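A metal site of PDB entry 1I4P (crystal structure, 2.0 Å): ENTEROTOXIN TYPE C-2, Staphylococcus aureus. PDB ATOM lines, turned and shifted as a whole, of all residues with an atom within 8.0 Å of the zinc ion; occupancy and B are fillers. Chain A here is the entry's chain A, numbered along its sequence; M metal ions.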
ATOM      1  N   ALA A  35      -6.246 -12.309 -16.158  1.00  0.00           N
ATOM      2  CA  ALA A  35      -6.784 -12.517 -17.509  1.00  0.00           C
ATOM      3  C   ALA A  35      -8.235 -13.008 -17.464  1.00  0.00           C
ATOM      4  O   ALA A  35      -8.670 -13.620 -16.487  1.00  0.00           O
ATOM      5  CB  ALA A  35      -5.921 -13.522 -18.286  1.00  0.00           C
ATOM      6  N   THR A  36      -8.998 -12.712 -18.524  1.00  0.00           N
ATOM      7  CA  THR A  36     -10.378 -13.149 -18.576  1.00  0.00           C
ATOM      8  C   THR A  36     -10.761 -13.866 -19.870  1.00  0.00           C
ATOM      9  O   THR A  36     -10.349 -13.492 -20.970  1.00  0.00           O
ATOM     10  CB  THR A  36     -11.396 -11.989 -18.289  1.00  0.00           C
ATOM     11  OG1 THR A  36     -12.250 -11.795 -19.429  1.00  0.00           O
ATOM     12  CG2 THR A  36     -10.666 -10.699 -17.973  1.00  0.00           C
ATOM     13  N   LYS A  37     -11.529 -14.948 -19.708  1.00  0.00           N
ATOM     14  CA  LYS A  37     -12.025 -15.754 -20.795  1.00  0.00           C
ATOM     15  C   LYS A  37     -11.008 -16.341 -21.764  1.00  0.00           C
ATOM     16  O   LYS A  37     -11.152 -16.228 -22.981  1.00  0.00           O
ATOM     17  CB  LYS A  37     -13.078 -14.968 -21.568  1.00  0.00           C
ATOM     18  CG  LYS A  37     -14.281 -14.579 -20.716  1.00  0.00           C
ATOM     19  CD  LYS A  37     -15.246 -13.697 -21.473  1.00  0.00           C
ATOM     20  CE  LYS A  37     -15.856 -14.438 -22.661  1.00  0.00           C
ATOM     21  NZ  LYS A  37     -16.788 -13.581 -23.451  1.00  0.00           N
ATOM     22  N   VAL A  38      -9.978 -16.993 -21.218  1.00  0.00           N
ATOM     23  CA  VAL A  38      -8.944 -17.625 -22.028  1.00  0.00           C
ATOM     24  C   VAL A  38      -9.032 -19.158 -21.935  1.00  0.00           C
ATOM     25  O   VAL A  38      -9.675 -19.697 -21.022  1.00  0.00           O
ATOM     26  CB  VAL A  38      -7.528 -17.166 -21.595  1.00  0.00           C
ATOM     27  CG1 VAL A  38      -7.344 -15.699 -21.895  1.00  0.00           C
ATOM     28  CG2 VAL A  38      -7.326 -17.427 -20.114  1.00  0.00           C
ATOM     29  N   VAL A  81     -13.156 -22.327 -20.775  1.00  0.00           N
ATOM     30  CA  VAL A  81     -12.908 -20.893 -20.940  1.00  0.00           C
ATOM     31  C   VAL A  81     -12.854 -20.410 -19.486  1.00  0.00           C
ATOM     32  O   VAL A  81     -13.859 -20.489 -18.763  1.00  0.00           O
ATOM     33  CB  VAL A  81     -14.054 -20.163 -21.693  1.00  0.00           C
ATOM     34  CG1 VAL A  81     -13.736 -18.670 -21.823  1.00  0.00           C
ATOM     35  CG2 VAL A  81     -14.253 -20.767 -23.076  1.00  0.00           C
ATOM     36  N   VAL A  82     -11.700 -19.919 -19.063  1.00  0.00           N
ATOM     37  CA  VAL A  82     -11.523 -19.500 -17.678  1.00  0.00           C
ATOM     38  C   VAL A  82     -11.039 -18.072 -17.447  1.00  0.00           C
ATOM     39  O   VAL A  82     -10.702 -17.337 -18.380  1.00  0.00           O
ATOM     40  CB  VAL A  82     -10.511 -20.424 -16.945  1.00  0.00           C
ATOM     41  CG1 VAL A  82     -10.985 -21.869 -16.973  1.00  0.00           C
ATOM     42  CG2 VAL A  82      -9.127 -20.297 -17.590  1.00  0.00           C
ATOM     43  N   ASP A  83     -11.001 -17.716 -16.170  1.00  0.00           N
ATOM     44  CA  ASP A  83     -10.504 -16.438 -15.700  1.00  0.00           C
ATOM     45  C   ASP A  83      -9.256 -16.806 -14.902  1.00  0.00           C
ATOM     46  O   ASP A  83      -9.223 -17.868 -14.281  1.00  0.00           O
ATOM     47  CB  ASP A  83     -11.513 -15.757 -14.780  1.00  0.00           C
ATOM     48  CG  ASP A  83     -12.785 -15.322 -15.505  1.00  0.00           C
ATOM     49  OD1 ASP A  83     -12.707 -15.062 -16.729  1.00  0.00           O
ATOM     50  OD2 ASP A  83     -13.855 -15.213 -14.856  1.00  0.00           O
ATOM     51  N   VAL A  84      -8.239 -15.964 -14.915  1.00  0.00           N
ATOM     52  CA  VAL A  84      -6.995 -16.250 -14.191  1.00  0.00           C
ATOM     53  C   VAL A  84      -6.557 -15.128 -13.236  1.00  0.00           C
ATOM     54  O   VAL A  84      -6.741 -13.947 -13.541  1.00  0.00           O
ATOM     55  CB  VAL A  84      -5.841 -16.507 -15.192  1.00  0.00           C
ATOM     56  CG1 VAL A  84      -4.556 -16.800 -14.434  1.00  0.00           C
ATOM     57  CG2 VAL A  84      -6.211 -17.644 -16.121  1.00  0.00           C
ATOM     58  N   THR A 116     -10.406 -20.256 -12.591  1.00  0.00           N
ATOM     59  CA  THR A 116     -11.826 -20.455 -12.313  1.00  0.00           C
ATOM     60  C   THR A 116     -12.650 -20.360 -13.621  1.00  0.00           C
ATOM     61  O   THR A 116     -12.334 -19.548 -14.492  1.00  0.00           O
ATOM     62  CB  THR A 116     -12.375 -19.380 -11.332  1.00  0.00           C
ATOM     63  OG1 THR A 116     -11.945 -18.080 -11.739  1.00  0.00           O
ATOM     64  CG2 THR A 116     -11.900 -19.661  -9.905  1.00  0.00           C
ATOM     65  N   LYS A 117     -13.686 -21.181 -13.752  1.00  0.00           N
ATOM     66  CA  LYS A 117     -14.519 -21.134 -14.949  1.00  0.00           C
ATOM     67  C   LYS A 117     -15.178 -19.766 -15.033  1.00  0.00           C
ATOM     68  O   LYS A 117     -15.586 -19.205 -14.014  1.00  0.00           O
ATOM     69  CB  LYS A 117     -15.606 -22.217 -14.892  1.00  0.00           C
ATOM     70  CG  LYS A 117     -15.047 -23.612 -14.746  1.00  0.00           C
ATOM     71  CD  LYS A 117     -16.129 -24.607 -14.344  1.00  0.00           C
ATOM     72  CE  LYS A 117     -15.518 -25.996 -14.139  1.00  0.00           C
ATOM     73  NZ  LYS A 117     -16.545 -26.990 -13.759  1.00  0.00           N
ATOM     74  N   HIS A 118     -15.278 -19.225 -16.241  1.00  0.00           N
ATOM     75  CA  HIS A 118     -15.899 -17.915 -16.452  1.00  0.00           C
ATOM     76  C   HIS A 118     -17.430 -17.950 -16.333  1.00  0.00           C
ATOM     77  O   HIS A 118     -18.010 -17.151 -15.589  1.00  0.00           O
ATOM     78  CB  HIS A 118     -15.516 -17.384 -17.829  1.00  0.00           C
ATOM     79  CG  HIS A 118     -16.397 -16.268 -18.312  1.00  0.00           C
ATOM     80  ND1 HIS A 118     -16.398 -15.021 -17.734  1.00  0.00           N
ATOM     81  CD2 HIS A 118     -17.306 -16.222 -19.309  1.00  0.00           C
ATOM     82  CE1 HIS A 118     -17.284 -14.251 -18.365  1.00  0.00           C
ATOM     83  NE2 HIS A 118     -17.843 -14.962 -19.317  1.00  0.00           N
ATOM     84  N   GLU A 119     -18.059 -18.874 -17.049  1.00  0.00           N
ATOM     85  CA  GLU A 119     -19.519 -18.962 -17.062  1.00  0.00           C
ATOM     86  C   GLU A 119     -20.204 -19.238 -15.730  1.00  0.00           C
ATOM     87  O   GLU A 119     -19.839 -20.157 -15.008  1.00  0.00           O
ATOM     88  CB  GLU A 119     -19.988 -20.011 -18.078  1.00  0.00           C
ATOM     89  CG  GLU A 119     -20.949 -19.441 -19.126  1.00  0.00           C
ATOM     90  CD  GLU A 119     -20.444 -18.143 -19.746  1.00  0.00           C
ATOM     91  OE1 GLU A 119     -20.631 -17.068 -19.144  1.00  0.00           O
ATOM     92  OE2 GLU A 119     -19.841 -18.206 -20.843  1.00  0.00           O
ATOM     93  N   GLY A 120     -21.198 -18.413 -15.428  1.00  0.00           N
ATOM     94  CA  GLY A 120     -21.965 -18.548 -14.207  1.00  0.00           C
ATOM     95  C   GLY A 120     -21.253 -18.151 -12.927  1.00  0.00           C
ATOM     96  O   GLY A 120     -21.779 -18.361 -11.830  1.00  0.00           O
ATOM     97  N   ASN A 121     -20.082 -17.547 -13.061  1.00  0.00           N
ATOM     98  CA  ASN A 121     -19.326 -17.180 -11.873  1.00  0.00           C
ATOM     99  C   ASN A 121     -19.323 -15.697 -11.530  1.00  0.00           C
ATOM    100  O   ASN A 121     -18.455 -15.250 -10.783  1.00  0.00           O
ATOM    101  CB  ASN A 121     -17.888 -17.698 -11.992  1.00  0.00           C
ATOM    102  CG  ASN A 121     -17.154 -17.702 -10.648  1.00  0.00           C
ATOM    103  OD1 ASN A 121     -17.699 -18.155  -9.630  1.00  0.00           O
ATOM    104  ND2 ASN A 121     -15.924 -17.215 -10.645  1.00  0.00           N
ATOM    105  N   HIS A 122     -20.263 -14.929 -12.052  1.00  0.00           N
ATOM    106  CA  HIS A 122     -20.298 -13.506 -11.725  1.00  0.00           C
ATOM    107  C   HIS A 122     -21.654 -13.071 -11.149  1.00  0.00           C
ATOM    108  O   HIS A 122     -22.640 -13.798 -11.268  1.00  0.00           O
ATOM    109  CB  HIS A 122     -19.922 -12.664 -12.950  1.00  0.00           C
ATOM    110  CG  HIS A 122     -18.521 -12.902 -13.423  1.00  0.00           C
ATOM    111  ND1 HIS A 122     -17.422 -12.690 -12.614  1.00  0.00           N
ATOM    112  CD2 HIS A 122     -18.031 -13.360 -14.597  1.00  0.00           C
ATOM    113  CE1 HIS A 122     -16.317 -12.999 -13.278  1.00  0.00           C
ATOM    114  NE2 HIS A 122     -16.667 -13.413 -14.475  1.00  0.00           N
ATOM    115  N   ASP A 150     -14.868  -9.816  -8.267  1.00  0.00           N
ATOM    116  CA  ASP A 150     -16.031  -9.891  -9.136  1.00  0.00           C
ATOM    117  C   ASP A 150     -16.484 -11.338  -9.306  1.00  0.00           C
ATOM    118  O   ASP A 150     -17.418 -11.621 -10.062  1.00  0.00           O
ATOM    119  CB  ASP A 150     -15.706  -9.294 -10.509  1.00  0.00           C
ATOM    120  CG  ASP A 150     -14.717 -10.129 -11.310  1.00  0.00           C
ATOM    121  OD1 ASP A 150     -13.744 -10.663 -10.724  1.00  0.00           O
ATOM    122  OD2 ASP A 150     -14.901 -10.254 -12.539  1.00  0.00           O
ATOM    123  N   LYS A 151     -15.834 -12.249  -8.581  1.00  0.00           N
ATOM    124  CA  LYS A 151     -16.157 -13.674  -8.683  1.00  0.00           C
ATOM    125  C   LYS A 151     -16.955 -14.233  -7.504  1.00  0.00           C
ATOM    126  O   LYS A 151     -16.630 -13.963  -6.346  1.00  0.00           O
ATOM    127  CB  LYS A 151     -14.866 -14.495  -8.828  1.00  0.00           C
ATOM    128  CG  LYS A 151     -13.961 -14.122  -9.997  1.00  0.00           C
ATOM    129  CD  LYS A 151     -12.676 -14.948  -9.962  1.00  0.00           C
ATOM    130  CE  LYS A 151     -11.698 -14.562 -11.069  1.00  0.00           C
ATOM    131  NZ  LYS A 151     -11.165 -13.164 -10.909  1.00  0.00           N
HETATM  132 ZN    ZN M   1     -15.211 -14.134 -16.000  1.00  0.00          ZN
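OD1 of Asp 83 lies within hydrogen-bond range of N of Lys 37, at 3.2 Å.
N of Asp 83 is in hydrogen-bond range of O of Thr 116.
A ring nitrogen (ND1) of His 122 lies within hydrogen-bond range of the backbone carbonyl oxygen of Asp 150 (2.8 Å).
A ring nitrogen (NE2) of His 118 lies close to the side-chain carboxylate (OE1) of Glu 119 (3.5 Å).
The backbone carbonyl oxygen of Val 81 lies within hydrogen-bond range of the backbone NH of His 118, at 3.2 Å.
Three residues have an atom within 4 Å of the zinc ion: Asp 83, His 118 and His 122.
The zinc ion is bound by OD2 of Asp 83 (2.1 Å).
The zinc ion is bound by NE2 of His 122 (2.2 Å).
The zinc ion is bound by ND1 of His 118, 2.3 Å away.
Slightly farther from the zinc ion lies OD1 of Asp 83 (2.8 Å).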
